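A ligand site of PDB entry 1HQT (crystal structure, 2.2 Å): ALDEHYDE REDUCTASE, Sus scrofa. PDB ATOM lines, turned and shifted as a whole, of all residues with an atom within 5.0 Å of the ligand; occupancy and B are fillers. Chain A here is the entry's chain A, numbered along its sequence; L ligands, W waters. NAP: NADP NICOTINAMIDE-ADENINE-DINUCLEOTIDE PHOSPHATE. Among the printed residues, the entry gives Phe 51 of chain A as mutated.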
ATOM      1  N   LEU A  20      30.490   0.887 -23.317  1.00  0.00           N
ATOM      2  CA  LEU A  20      29.370   0.225 -22.667  1.00  0.00           C
ATOM      3  C   LEU A  20      28.222   1.186 -22.374  1.00  0.00           C
ATOM      4  O   LEU A  20      28.357   2.099 -21.549  1.00  0.00           O
ATOM      5  CB  LEU A  20      29.827  -0.464 -21.381  1.00  0.00           C
ATOM      6  CG  LEU A  20      28.762  -1.210 -20.564  1.00  0.00           C
ATOM      7  CD1 LEU A  20      28.266  -2.421 -21.324  1.00  0.00           C
ATOM      8  CD2 LEU A  20      29.338  -1.651 -19.235  1.00  0.00           C
ATOM      9  N   GLY A  21      27.095   0.992 -23.042  1.00  0.00           N
ATOM     10  CA  GLY A  21      25.929   1.831 -22.801  1.00  0.00           C
ATOM     11  C   GLY A  21      25.274   1.393 -21.506  1.00  0.00           C
ATOM     12  O   GLY A  21      25.428   0.250 -21.091  1.00  0.00           O
ATOM     13  N   THR A  22      24.554   2.304 -20.851  1.00  0.00           N
ATOM     14  CA  THR A  22      23.908   1.968 -19.589  1.00  0.00           C
ATOM     15  C   THR A  22      22.462   2.455 -19.451  1.00  0.00           C
ATOM     16  O   THR A  22      21.935   2.524 -18.347  1.00  0.00           O
ATOM     17  CB  THR A  22      24.707   2.508 -18.372  1.00  0.00           C
ATOM     18  OG1 THR A  22      24.831   3.936 -18.460  1.00  0.00           O
ATOM     19  CG2 THR A  22      26.098   1.870 -18.325  1.00  0.00           C
ATOM     20  N   TRP A  23      21.825   2.795 -20.574  1.00  0.00           N
ATOM     21  CA  TRP A  23      20.446   3.254 -20.533  1.00  0.00           C
ATOM     22  C   TRP A  23      19.538   2.103 -20.158  1.00  0.00           C
ATOM     23  O   TRP A  23      19.567   1.050 -20.811  1.00  0.00           O
ATOM     24  CB  TRP A  23      19.996   3.839 -21.873  1.00  0.00           C
ATOM     25  CG  TRP A  23      18.520   4.186 -21.916  1.00  0.00           C
ATOM     26  CD1 TRP A  23      17.747   4.603 -20.872  1.00  0.00           C
ATOM     27  CD2 TRP A  23      17.675   4.189 -23.068  1.00  0.00           C
ATOM     28  NE1 TRP A  23      16.472   4.864 -21.300  1.00  0.00           N
ATOM     29  CE2 TRP A  23      16.398   4.620 -22.649  1.00  0.00           C
ATOM     30  CE3 TRP A  23      17.861   3.873 -24.433  1.00  0.00           C
ATOM     31  CZ2 TRP A  23      15.306   4.745 -23.531  1.00  0.00           C
ATOM     32  CZ3 TRP A  23      16.780   3.996 -25.301  1.00  0.00           C
ATOM     33  CH2 TRP A  23      15.522   4.422 -24.846  1.00  0.00           C
ATOM     34  N   ASP A  46      29.529   4.635 -21.031  1.00  0.00           N
ATOM     35  CA  ASP A  46      28.636   5.742 -21.348  1.00  0.00           C
ATOM     36  C   ASP A  46      27.547   5.801 -20.272  1.00  0.00           C
ATOM     37  O   ASP A  46      26.829   4.827 -20.076  1.00  0.00           O
ATOM     38  CB  ASP A  46      28.004   5.567 -22.730  1.00  0.00           C
ATOM     39  CG  ASP A  46      27.164   6.761 -23.143  1.00  0.00           C
ATOM     40  OD1 ASP A  46      26.010   6.875 -22.683  1.00  0.00           O
ATOM     41  OD2 ASP A  46      27.673   7.589 -23.910  1.00  0.00           O
ATOM     42  N   CYS A  47      27.433   6.955 -19.607  1.00  0.00           N
ATOM     43  CA  CYS A  47      26.452   7.144 -18.537  1.00  0.00           C
ATOM     44  C   CYS A  47      25.576   8.383 -18.738  1.00  0.00           C
ATOM     45  O   CYS A  47      25.809   9.183 -19.645  1.00  0.00           O
ATOM     46  CB  CYS A  47      27.166   7.290 -17.174  1.00  0.00           C
ATOM     47  SG  CYS A  47      28.594   6.224 -16.908  1.00  0.00           S
ATOM     48  N   PHE A  51      19.375   8.362 -16.378  1.00  0.00           N
ATOM     49  CA  PHE A  51      19.215   6.913 -16.333  1.00  0.00           C
ATOM     50  C   PHE A  51      18.979   6.444 -14.904  1.00  0.00           C
ATOM     51  O   PHE A  51      18.543   5.321 -14.680  1.00  0.00           O
ATOM     52  CB  PHE A  51      20.449   6.199 -16.902  1.00  0.00           C
ATOM     53  CG  PHE A  51      20.728   6.493 -18.358  1.00  0.00           C
ATOM     54  CD1 PHE A  51      19.717   6.976 -19.191  1.00  0.00           C
ATOM     55  CD2 PHE A  51      21.997   6.279 -18.884  1.00  0.00           C
ATOM     56  CE1 PHE A  51      19.972   7.244 -20.541  1.00  0.00           C
ATOM     57  CE2 PHE A  51      22.271   6.536 -20.229  1.00  0.00           C
ATOM     58  CZ  PHE A  51      21.254   7.027 -21.064  1.00  0.00           C
ATOM     59  N   LYS A  81      25.941  12.832 -19.110  1.00  0.00           N
ATOM     60  CA  LYS A  81      25.194  13.911 -19.740  1.00  0.00           C
ATOM     61  C   LYS A  81      24.419  14.814 -18.799  1.00  0.00           C
ATOM     62  O   LYS A  81      23.966  14.391 -17.728  1.00  0.00           O
ATOM     63  CB  LYS A  81      24.227  13.326 -20.766  1.00  0.00           C
ATOM     64  CG  LYS A  81      24.811  12.208 -21.603  1.00  0.00           C
ATOM     65  CD  LYS A  81      23.818  11.690 -22.633  1.00  0.00           C
ATOM     66  CE  LYS A  81      24.425  10.555 -23.453  1.00  0.00           C
ATOM     67  NZ  LYS A  81      24.764   9.392 -22.606  1.00  0.00           N
ATOM     68  N   HIS A 114      22.459  16.508 -22.854  1.00  0.00           N
ATOM     69  CA  HIS A 114      21.582  15.416 -23.287  1.00  0.00           C
ATOM     70  C   HIS A 114      20.611  15.745 -24.407  1.00  0.00           C
ATOM     71  O   HIS A 114      20.379  14.927 -25.295  1.00  0.00           O
ATOM     72  CB  HIS A 114      20.842  14.851 -22.072  1.00  0.00           C
ATOM     73  CG  HIS A 114      20.642  13.367 -22.143  1.00  0.00           C
ATOM     74  ND1 HIS A 114      20.700  12.552 -21.033  1.00  0.00           N
ATOM     75  CD2 HIS A 114      20.364  12.552 -23.189  1.00  0.00           C
ATOM     76  CE1 HIS A 114      20.460  11.308 -21.384  1.00  0.00           C
ATOM     77  NE2 HIS A 114      20.249  11.284 -22.687  1.00  0.00           N
ATOM     78  N   TRP A 115      20.031  16.944 -24.354  1.00  0.00           N
ATOM     79  CA  TRP A 115      19.125  17.410 -25.398  1.00  0.00           C
ATOM     80  C   TRP A 115      19.319  18.906 -25.547  1.00  0.00           C
ATOM     81  O   TRP A 115      19.745  19.589 -24.601  1.00  0.00           O
ATOM     82  CB  TRP A 115      17.669  17.112 -25.071  1.00  0.00           C
ATOM     83  CG  TRP A 115      17.291  15.666 -25.094  1.00  0.00           C
ATOM     84  CD1 TRP A 115      17.346  14.787 -24.062  1.00  0.00           C
ATOM     85  CD2 TRP A 115      16.752  14.945 -26.218  1.00  0.00           C
ATOM     86  NE1 TRP A 115      16.874  13.552 -24.454  1.00  0.00           N
ATOM     87  CE2 TRP A 115      16.511  13.625 -25.773  1.00  0.00           C
ATOM     88  CE3 TRP A 115      16.465  15.289 -27.545  1.00  0.00           C
ATOM     89  CZ2 TRP A 115      15.982  12.639 -26.626  1.00  0.00           C
ATOM     90  CZ3 TRP A 115      15.938  14.309 -28.376  1.00  0.00           C
ATOM     91  CH2 TRP A 115      15.710  13.000 -27.918  1.00  0.00           C
ATOM     92  N   SER A 163      24.406  16.044 -27.542  1.00  0.00           N
ATOM     93  CA  SER A 163      23.566  14.870 -27.710  1.00  0.00           C
ATOM     94  C   SER A 163      22.226  15.272 -28.294  1.00  0.00           C
ATOM     95  O   SER A 163      21.546  16.146 -27.754  1.00  0.00           O
ATOM     96  CB  SER A 163      23.324  14.181 -26.376  1.00  0.00           C
ATOM     97  OG  SER A 163      22.287  13.229 -26.525  1.00  0.00           O
ATOM     98  N   ASN A 164      21.853  14.630 -29.390  1.00  0.00           N
ATOM     99  CA  ASN A 164      20.586  14.909 -30.063  1.00  0.00           C
ATOM    100  C   ASN A 164      20.515  16.318 -30.620  1.00  0.00           C
ATOM    101  O   ASN A 164      19.458  16.939 -30.598  1.00  0.00           O
ATOM    102  CB  ASN A 164      19.409  14.667 -29.118  1.00  0.00           C
ATOM    103  CG  ASN A 164      19.324  13.240 -28.647  1.00  0.00           C
ATOM    104  OD1 ASN A 164      19.200  12.326 -29.459  1.00  0.00           O
ATOM    105  ND2 ASN A 164      19.386  13.039 -27.343  1.00  0.00           N
ATOM    106  N   GLN A 185      26.602  12.838 -30.028  1.00  0.00           N
ATOM    107  CA  GLN A 185      26.001  11.532 -29.774  1.00  0.00           C
ATOM    108  C   GLN A 185      24.556  11.518 -30.261  1.00  0.00           C
ATOM    109  O   GLN A 185      23.733  12.321 -29.804  1.00  0.00           O
ATOM    110  CB  GLN A 185      26.064  11.173 -28.280  1.00  0.00           C
ATOM    111  CG  GLN A 185      25.224   9.944 -27.921  1.00  0.00           C
ATOM    112  CD  GLN A 185      25.685   9.201 -26.679  1.00  0.00           C
ATOM    113  OE1 GLN A 185      24.922   8.458 -26.080  1.00  0.00           O
ATOM    114  NE2 GLN A 185      26.951   9.380 -26.296  1.00  0.00           N
ATOM    115  N   TYR A 211      24.219   5.849 -30.405  1.00  0.00           N
ATOM    116  CA  TYR A 211      23.536   5.139 -29.337  1.00  0.00           C
ATOM    117  C   TYR A 211      22.436   4.330 -30.036  1.00  0.00           C
ATOM    118  O   TYR A 211      22.042   4.677 -31.153  1.00  0.00           O
ATOM    119  CB  TYR A 211      22.984   6.105 -28.260  1.00  0.00           C
ATOM    120  CG  TYR A 211      21.834   7.039 -28.612  1.00  0.00           C
ATOM    121  CD1 TYR A 211      22.025   8.425 -28.642  1.00  0.00           C
ATOM    122  CD2 TYR A 211      20.538   6.550 -28.821  1.00  0.00           C
ATOM    123  CE1 TYR A 211      20.954   9.302 -28.851  1.00  0.00           C
ATOM    124  CE2 TYR A 211      19.467   7.427 -29.030  1.00  0.00           C
ATOM    125  CZ  TYR A 211      19.686   8.801 -29.032  1.00  0.00           C
ATOM    126  OH  TYR A 211      18.642   9.679 -29.203  1.00  0.00           O
ATOM    127  N   SER A 212      21.982   3.256 -29.409  1.00  0.00           N
ATOM    128  CA  SER A 212      20.977   2.370 -30.003  1.00  0.00           C
ATOM    129  C   SER A 212      21.464   1.818 -31.348  1.00  0.00           C
ATOM    130  O   SER A 212      20.716   1.782 -32.331  1.00  0.00           O
ATOM    131  CB  SER A 212      19.651   3.106 -30.215  1.00  0.00           C
ATOM    132  OG  SER A 212      18.965   3.263 -28.994  1.00  0.00           O
ATOM    133  N   PRO A 213      22.719   1.339 -31.403  1.00  0.00           N
ATOM    134  CA  PRO A 213      23.301   0.788 -32.629  1.00  0.00           C
ATOM    135  C   PRO A 213      22.651  -0.506 -33.103  1.00  0.00           C
ATOM    136  O   PRO A 213      22.766  -0.879 -34.261  1.00  0.00           O
ATOM    137  CB  PRO A 213      24.764   0.587 -32.241  1.00  0.00           C
ATOM    138  CG  PRO A 213      24.637   0.148 -30.822  1.00  0.00           C
ATOM    139  CD  PRO A 213      23.622   1.138 -30.264  1.00  0.00           C
ATOM    140  N   LEU A 214      21.976  -1.197 -32.198  1.00  0.00           N
ATOM    141  CA  LEU A 214      21.314  -2.442 -32.549  1.00  0.00           C
ATOM    142  C   LEU A 214      19.842  -2.154 -32.832  1.00  0.00           C
ATOM    143  O   LEU A 214      19.104  -3.019 -33.279  1.00  0.00           O
ATOM    144  CB  LEU A 214      21.425  -3.450 -31.403  1.00  0.00           C
ATOM    145  CG  LEU A 214      22.792  -3.605 -30.738  1.00  0.00           C
ATOM    146  CD1 LEU A 214      22.674  -4.600 -29.613  1.00  0.00           C
ATOM    147  CD2 LEU A 214      23.838  -4.049 -31.740  1.00  0.00           C
ATOM    148  N   GLY A 215      19.435  -0.920 -32.575  1.00  0.00           N
ATOM    149  CA  GLY A 215      18.058  -0.536 -32.776  1.00  0.00           C
ATOM    150  C   GLY A 215      17.330  -0.505 -31.437  1.00  0.00           C
ATOM    151  O   GLY A 215      16.116  -0.324 -31.385  1.00  0.00           O
ATOM    152  N   SER A 216      18.098  -0.665 -30.354  1.00  0.00           N
ATOM    153  CA  SER A 216      17.569  -0.658 -28.993  1.00  0.00           C
ATOM    154  C   SER A 216      16.707  -1.887 -28.692  1.00  0.00           C
ATOM    155  O   SER A 216      16.137  -2.005 -27.608  1.00  0.00           O
ATOM    156  CB  SER A 216      16.758   0.625 -28.750  1.00  0.00           C
ATOM    157  OG  SER A 216      16.296   0.690 -27.420  1.00  0.00           O
ATOM    158  N   SER A 217      16.624  -2.795 -29.659  1.00  0.00           N
ATOM    159  CA  SER A 217      15.849  -4.036 -29.522  1.00  0.00           C
ATOM    160  C   SER A 217      14.359  -3.813 -29.325  1.00  0.00           C
ATOM    161  O   SER A 217      13.532  -4.567 -29.854  1.00  0.00           O
ATOM    162  CB  SER A 217      16.392  -4.882 -28.365  1.00  0.00           C
ATOM    163  OG  SER A 217      17.695  -5.362 -28.656  1.00  0.00           O
ATOM    164  N   ASP A 218      14.000  -2.779 -28.576  1.00  0.00           N
ATOM    165  CA  ASP A 218      12.601  -2.450 -28.308  1.00  0.00           C
ATOM    166  C   ASP A 218      12.468  -1.171 -27.477  1.00  0.00           C
ATOM    167  O   ASP A 218      11.404  -0.889 -26.934  1.00  0.00           O
ATOM    168  CB  ASP A 218      11.905  -3.617 -27.597  1.00  0.00           C
ATOM    169  CG  ASP A 218      12.683  -4.115 -26.392  1.00  0.00           C
ATOM    170  OD1 ASP A 218      13.819  -4.591 -26.582  1.00  0.00           O
ATOM    171  OD2 ASP A 218      12.152  -4.033 -25.267  1.00  0.00           O
ATOM    172  N   SER A 245      27.355 -13.008 -34.318  1.00  0.00           N
ATOM    173  CA  SER A 245      25.948 -12.713 -34.064  1.00  0.00           C
ATOM    174  C   SER A 245      25.460 -11.489 -34.845  1.00  0.00           C
ATOM    175  O   SER A 245      26.246 -10.654 -35.289  1.00  0.00           O
ATOM    176  CB  SER A 245      25.711 -12.502 -32.562  1.00  0.00           C
ATOM    177  OG  SER A 245      26.292 -11.291 -32.121  1.00  0.00           O
ATOM    178  N   ALA A 247      24.085  -8.780 -33.902  1.00  0.00           N
ATOM    179  CA  ALA A 247      24.503  -7.536 -33.275  1.00  0.00           C
ATOM    180  C   ALA A 247      25.965  -7.205 -33.578  1.00  0.00           C
ATOM    181  O   ALA A 247      26.326  -6.046 -33.780  1.00  0.00           O
ATOM    182  CB  ALA A 247      24.287  -7.599 -31.770  1.00  0.00           C
ATOM    183  N   ILE A 262      28.197   2.649 -28.392  1.00  0.00           N
ATOM    184  CA  ILE A 262      28.187   2.375 -26.966  1.00  0.00           C
ATOM    185  C   ILE A 262      27.119   1.357 -26.587  1.00  0.00           C
ATOM    186  O   ILE A 262      26.388   1.567 -25.614  1.00  0.00           O
ATOM    187  CB  ILE A 262      27.945   3.669 -26.163  1.00  0.00           C
ATOM    188  CG1 ILE A 262      26.638   4.329 -26.623  1.00  0.00           C
ATOM    189  CG2 ILE A 262      29.119   4.633 -26.360  1.00  0.00           C
ATOM    190  CD1 ILE A 262      26.344   5.640 -25.948  1.00  0.00           C
ATOM    191  N   PRO A 263      27.035   0.232 -27.325  1.00  0.00           N
ATOM    192  CA  PRO A 263      26.040  -0.828 -27.073  1.00  0.00           C
ATOM    193  C   PRO A 263      25.754  -1.101 -25.608  1.00  0.00           C
ATOM    194  O   PRO A 263      26.660  -1.263 -24.798  1.00  0.00           O
ATOM    195  CB  PRO A 263      26.657  -2.047 -27.750  1.00  0.00           C
ATOM    196  CG  PRO A 263      28.131  -1.766 -27.710  1.00  0.00           C
ATOM    197  CD  PRO A 263      28.156  -0.310 -28.104  1.00  0.00           C
ATOM    198  N   LYS A 264      24.468  -1.169 -25.276  1.00  0.00           N
ATOM    199  CA  LYS A 264      24.053  -1.441 -23.907  1.00  0.00           C
ATOM    200  C   LYS A 264      23.687  -2.897 -23.731  1.00  0.00           C
ATOM    201  O   LYS A 264      23.068  -3.500 -24.601  1.00  0.00           O
ATOM    202  CB  LYS A 264      22.849  -0.558 -23.530  1.00  0.00           C
ATOM    203  CG  LYS A 264      22.241  -0.872 -22.153  1.00  0.00           C
ATOM    204  CD  LYS A 264      21.308  -2.095 -22.193  1.00  0.00           C
ATOM    205  CE  LYS A 264      20.699  -2.387 -20.827  1.00  0.00           C
ATOM    206  NZ  LYS A 264      19.764  -3.547 -20.854  1.00  0.00           N
ATOM    207  N   SER A 265      24.067  -3.452 -22.585  1.00  0.00           N
ATOM    208  CA  SER A 265      23.756  -4.846 -22.277  1.00  0.00           C
ATOM    209  C   SER A 265      24.116  -5.193 -20.836  1.00  0.00           C
ATOM    210  O   SER A 265      25.120  -4.723 -20.314  1.00  0.00           O
ATOM    211  CB  SER A 265      24.496  -5.788 -23.218  1.00  0.00           C
ATOM    212  OG  SER A 265      24.136  -7.124 -22.942  1.00  0.00           O
ATOM    213  N   VAL A 266      23.261  -5.999 -20.203  1.00  0.00           N
ATOM    214  CA  VAL A 266      23.500  -6.447 -18.831  1.00  0.00           C
ATOM    215  C   VAL A 266      23.507  -7.982 -18.847  1.00  0.00           C
ATOM    216  O   VAL A 266      23.422  -8.638 -17.811  1.00  0.00           O
ATOM    217  CB  VAL A 266      22.399  -5.950 -17.873  1.00  0.00           C
ATOM    218  CG1 VAL A 266      22.422  -4.423 -17.807  1.00  0.00           C
ATOM    219  CG2 VAL A 266      21.035  -6.468 -18.340  1.00  0.00           C
ATOM    220  N   THR A 267      23.600  -8.520 -20.061  1.00  0.00           N
ATOM    221  CA  THR A 267      23.626  -9.962 -20.296  1.00  0.00           C
ATOM    222  C   THR A 267      25.077 -10.407 -20.430  1.00  0.00           C
ATOM    223  O   THR A 267      25.777  -9.989 -21.352  1.00  0.00           O
ATOM    224  CB  THR A 267      22.877 -10.287 -21.593  1.00  0.00           C
ATOM    225  OG1 THR A 267      21.510  -9.881 -21.458  1.00  0.00           O
ATOM    226  CG2 THR A 267      22.966 -11.781 -21.896  1.00  0.00           C
ATOM    227  N   ARG A 270      26.622 -11.364 -23.944  1.00  0.00           N
ATOM    228  CA  ARG A 270      26.614 -10.367 -25.010  1.00  0.00           C
ATOM    229  C   ARG A 270      27.680  -9.294 -24.796  1.00  0.00           C
ATOM    230  O   ARG A 270      28.266  -8.781 -25.765  1.00  0.00           O
ATOM    231  CB  ARG A 270      25.230  -9.705 -25.097  1.00  0.00           C
ATOM    232  CG  ARG A 270      24.132 -10.631 -25.583  1.00  0.00           C
ATOM    233  CD  ARG A 270      22.769  -9.987 -25.394  1.00  0.00           C
ATOM    234  NE  ARG A 270      21.692 -10.772 -25.972  1.00  0.00           N
ATOM    235  CZ  ARG A 270      20.410 -10.441 -25.921  1.00  0.00           C
ATOM    236  NH1 ARG A 270      20.029  -9.330 -25.299  1.00  0.00           N
ATOM    237  NH2 ARG A 270      19.491 -11.218 -26.476  1.00  0.00           N
ATOM    238  N   GLN A 273      30.851 -10.092 -26.482  1.00  0.00           N
ATOM    239  CA  GLN A 273      30.621 -10.152 -27.927  1.00  0.00           C
ATOM    240  C   GLN A 273      30.532  -8.771 -28.572  1.00  0.00           C
ATOM    241  O   GLN A 273      31.036  -8.566 -29.670  1.00  0.00           O
ATOM    242  CB  GLN A 273      29.320 -10.912 -28.232  1.00  0.00           C
ATOM    243  CG  GLN A 273      29.311 -12.397 -27.856  1.00  0.00           C
ATOM    244  CD  GLN A 273      27.946 -13.036 -28.049  1.00  0.00           C
ATOM    245  OE1 GLN A 273      26.933 -12.511 -27.574  1.00  0.00           O
ATOM    246  NE2 GLN A 273      27.905 -14.170 -28.734  1.00  0.00           N
ATOM    247  N   ASN A 274      29.893  -7.829 -27.873  1.00  0.00           N
ATOM    248  CA  ASN A 274      29.700  -6.481 -28.392  1.00  0.00           C
ATOM    249  C   ASN A 274      30.974  -5.680 -28.580  1.00  0.00           C
ATOM    250  O   ASN A 274      30.984  -4.690 -29.299  1.00  0.00           O
ATOM    251  CB  ASN A 274      28.728  -5.708 -27.500  1.00  0.00           C
ATOM    252  CG  ASN A 274      27.344  -6.332 -27.501  1.00  0.00           C
ATOM    253  OD1 ASN A 274      26.996  -7.099 -28.398  1.00  0.00           O
ATOM    254  ND2 ASN A 274      26.545  -6.002 -26.489  1.00  0.00           N
ATOM    255  N   ILE A 300      14.121   6.448 -31.450  1.00  0.00           N
ATOM    256  CA  ILE A 300      14.171   7.061 -30.122  1.00  0.00           C
ATOM    257  C   ILE A 300      13.423   8.365 -29.882  1.00  0.00           C
ATOM    258  O   ILE A 300      13.977   9.330 -29.355  1.00  0.00           O
ATOM    259  CB  ILE A 300      15.643   7.240 -29.683  1.00  0.00           C
ATOM    260  CG1 ILE A 300      16.427   5.956 -29.965  1.00  0.00           C
ATOM    261  CG2 ILE A 300      15.713   7.552 -28.198  1.00  0.00           C
ATOM    262  CD1 ILE A 300      15.867   4.725 -29.271  1.00  0.00           C
HETATM  263  PA  NAP L   1      21.215  -0.791 -28.092  1.00  0.00           P
HETATM  264  O1A NAP L   1      22.517  -0.790 -27.489  1.00  0.00           O
HETATM  265  O2A NAP L   1      21.099  -0.725 -29.593  1.00  0.00           O
HETATM  266  O5B NAP L   1      20.319  -2.090 -27.669  1.00  0.00           O
HETATM  267  C5B NAP L   1      20.174  -2.500 -26.306  1.00  0.00           C
HETATM  268  C4B NAP L   1      19.262  -3.709 -26.277  1.00  0.00           C
HETATM  269  O4B NAP L   1      19.885  -4.728 -27.067  1.00  0.00           O
HETATM  270  C3B NAP L   1      19.046  -4.247 -24.908  1.00  0.00           C
HETATM  271  O3B NAP L   1      17.682  -4.715 -24.740  1.00  0.00           O
HETATM  272  C2B NAP L   1      20.017  -5.409 -24.833  1.00  0.00           C
HETATM  273  O2B NAP L   1      19.563  -6.505 -24.021  1.00  0.00           O
HETATM  274  C1B NAP L   1      20.103  -5.900 -26.273  1.00  0.00           C
HETATM  275  N9A NAP L   1      21.440  -6.416 -26.712  1.00  0.00           N
HETATM  276  C8A NAP L   1      22.709  -6.017 -26.308  1.00  0.00           C
HETATM  277  N7A NAP L   1      23.665  -6.677 -26.887  1.00  0.00           N
HETATM  278  C5A NAP L   1      23.034  -7.559 -27.721  1.00  0.00           C
HETATM  279  C6A NAP L   1      23.513  -8.524 -28.610  1.00  0.00           C
HETATM  280  N6A NAP L   1      24.809  -8.736 -28.766  1.00  0.00           N
HETATM  281  N1A NAP L   1      22.604  -9.269 -29.327  1.00  0.00           N
HETATM  282  C2A NAP L   1      21.278  -9.055 -29.169  1.00  0.00           C
HETATM  283  N3A NAP L   1      20.734  -8.148 -28.342  1.00  0.00           N
HETATM  284  C4A NAP L   1      21.673  -7.421 -27.639  1.00  0.00           C
HETATM  285  O3  NAP L   1      20.251   0.346 -27.482  1.00  0.00           O
HETATM  286  PN  NAP L   1      20.322   1.548 -26.433  1.00  0.00           P
HETATM  287  O1N NAP L   1      19.085   2.315 -26.630  1.00  0.00           O
HETATM  288  O2N NAP L   1      20.513   0.880 -25.105  1.00  0.00           O
HETATM  289  O5D NAP L   1      21.659   2.411 -26.683  1.00  0.00           O
HETATM  290  C5D NAP L   1      22.905   2.073 -26.049  1.00  0.00           C
HETATM  291  C4D NAP L   1      23.430   3.159 -25.100  1.00  0.00           C
HETATM  292  O4D NAP L   1      23.276   4.446 -25.715  1.00  0.00           O
HETATM  293  C3D NAP L   1      22.659   3.313 -23.809  1.00  0.00           C
HETATM  294  O3D NAP L   1      22.879   2.297 -22.831  1.00  0.00           O
HETATM  295  C2D NAP L   1      23.095   4.674 -23.327  1.00  0.00           C
HETATM  296  O2D NAP L   1      24.360   4.691 -22.692  1.00  0.00           O
HETATM  297  C1D NAP L   1      23.108   5.450 -24.698  1.00  0.00           C
HETATM  298  N1N NAP L   1      21.875   6.241 -24.925  1.00  0.00           N
HETATM  299  C2N NAP L   1      22.122   7.619 -25.116  1.00  0.00           C
HETATM  300  C3N NAP L   1      20.984   8.469 -25.334  1.00  0.00           C
HETATM  301  C7N NAP L   1      21.146   9.917 -25.556  1.00  0.00           C
HETATM  302  O7N NAP L   1      20.180  10.673 -25.752  1.00  0.00           O
HETATM  303  N7N NAP L   1      22.372  10.472 -25.550  1.00  0.00           N
HETATM  304  C4N NAP L   1      19.691   7.900 -25.348  1.00  0.00           C
HETATM  305  C5N NAP L   1      19.472   6.569 -25.158  1.00  0.00           C
HETATM  306  C6N NAP L   1      20.548   5.733 -24.945  1.00  0.00           C
HETATM  307  P2B NAP L   1      20.315  -6.912 -22.673  1.00  0.00           P
HETATM  308  O1X NAP L   1      20.721  -5.705 -21.906  1.00  0.00           O
HETATM  309  O2X NAP L   1      19.248  -7.705 -22.066  1.00  0.00           O
HETATM  310  O3X NAP L   1      21.431  -7.740 -23.165  1.00  0.00           O
HETATM  311  O   HOH W   1      16.921  -5.682 -21.900  1.00  0.00           O
HETATM  312  O   HOH W   2      25.636 -11.510 -29.592  1.00  0.00           O
HETATM  313  O   HOH W   3      18.323  -7.170 -19.555  1.00  0.00           O
HETATM  314  O   HOH W   4      18.820 -11.013 -30.684  1.00  0.00           O
HETATM  315  O   HOH W   5      22.738 -10.517 -32.034  1.00  0.00           O
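The side-chain hydroxyl (OG1) of Thr 22 lies within hydrogen-bond range of the backbone carbonyl oxygen (O) of Asp 46. The side-chain carboxylate (OD1) of Asp 46 is in salt-bridge range of the side-chain amino group (NZ) of Lys 81, 2.8 Å away. The side-chain amide nitrogen (NE2) of Gln 185 is in hydrogen-bond range of the side-chain carboxylate (OD2) of Asp 46, 3.1 Å away. OG of Ser 265 sits at hydrogen-bond distance from N of Thr 267 (3.2 Å). The side-chain amide nitrogen (ND2) of Asn 164 lies within hydrogen-bond range of the side-chain hydroxyl (OG) of Ser 163 (3.0 Å). NZ of Lys 81 sits at hydrogen-bond distance from O of Cys 47 (3.1 Å). The side-chain hydroxyl (OH) of Tyr 211 sits at hydrogen-bond distance from the side-chain amide oxygen (OD1) of Asn 164. O of Gln 185 sits at hydrogen-bond distance from N of Asn 164.
The backbone NH (N) of Trp 23 sits at hydrogen-bond distance from an oxygen (O3D) of the ligand, at 2.5 Å. O5D of the ligand lies within hydrogen-bond range of N of Ser 212. The side-chain hydroxyl (OG) of Ser 212 sits at hydrogen-bond distance from an oxygen (O1N) of the ligand, 2.5 Å away. An oxygen (O1A) of the ligand sits at hydrogen-bond distance from the backbone NH (N) of Lys 264 (3.0 Å). The side-chain amino group (NZ) of Lys 264 is in salt-bridge range of an oxygen (O1X) of the ligand. An oxygen (O3D) of the ligand is in hydrogen-bond range of the backbone NH (N) of Thr 22 (2.6 Å). OD1 of Asp 46 lies within hydrogen-bond range of O2D of the ligand, 2.7 Å away. OG1 of Thr 267 is in hydrogen-bond range of O3X of the ligand. N6A of the ligand is in hydrogen-bond range of OD1 of Asn 274 (2.8 Å). The side-chain hydroxyl (OG) of Ser 217 is in hydrogen-bond range of an oxygen (O4B) of the ligand (2.8 Å). An oxygen (O3X) of the ligand is in hydrogen-bond range of the side-chain hydroxyl (OG) of Ser 265, at 2.8 Å. An oxygen (O2A) of the ligand lies within hydrogen-bond range of the backbone NH (N) of Leu 214. N7N of the ligand lies within hydrogen-bond range of OG of Ser 163 (2.9 Å). The side-chain amide nitrogen (ND2) of Asn 164 lies within hydrogen-bond range of an oxygen (O7N) of the ligand (3.0 Å). The guanidinium group (NH1) of Arg 270 lies within salt-bridge range of an oxygen (O3X) of the ligand, 3.0 Å away. O1X of the ligand lies within hydrogen-bond range of N of Val 266 (3.1 Å). OE1 of Gln 185 lies close to N7N of the ligand (3.3 Å). The backbone NH (N) of Ser 216 lies within hydrogen-bond range of an oxygen (O2A) of the ligand. The side-chain hydroxyl of Ser 216 sits at hydrogen-bond distance from an oxygen (O1N) of the ligand (3.3 Å). NE2 of His 114 lies within hydrogen-bond range of O7N of the ligand, at 3.1 Å. N of Gly 215 is in hydrogen-bond range of O2A of the ligand (3.4 Å).
The backbone nitrogen of Pro 213 lies close to an oxygen (O2A) of the ligand, 3.2 Å away. Merely in contact with the ligand: Gly 21 (2.9 Å), Lys 81 (2.9 Å), Tyr 211 (3.1 Å), Ala 247 (3.3 Å), Ile 262 (3.3 Å), Pro 263 (3.5 Å) and Phe 51 (3.7 Å). Hydrophobic or aromatic side chains within 4 Å of the ligand: Trp 23, Phe 51, His 114, Tyr 211, Pro 213, Leu 214, Ala 247, Ile 262 and Val 266. The nearest printed residue that does not touch the ligand is Asp 218 (4.3 Å).
Water W5 lies within hydrogen-bond range of the backbone NH of Ala 247 (2.9 Å) and a nitrogen (N1A) of the ligand (3.0 Å). Water W2 lies within hydrogen-bond range of OE1 of Gln 273 (2.6 Å), OG of Ser 245 (2.6 Å) and N6A of the ligand (3.0 Å).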
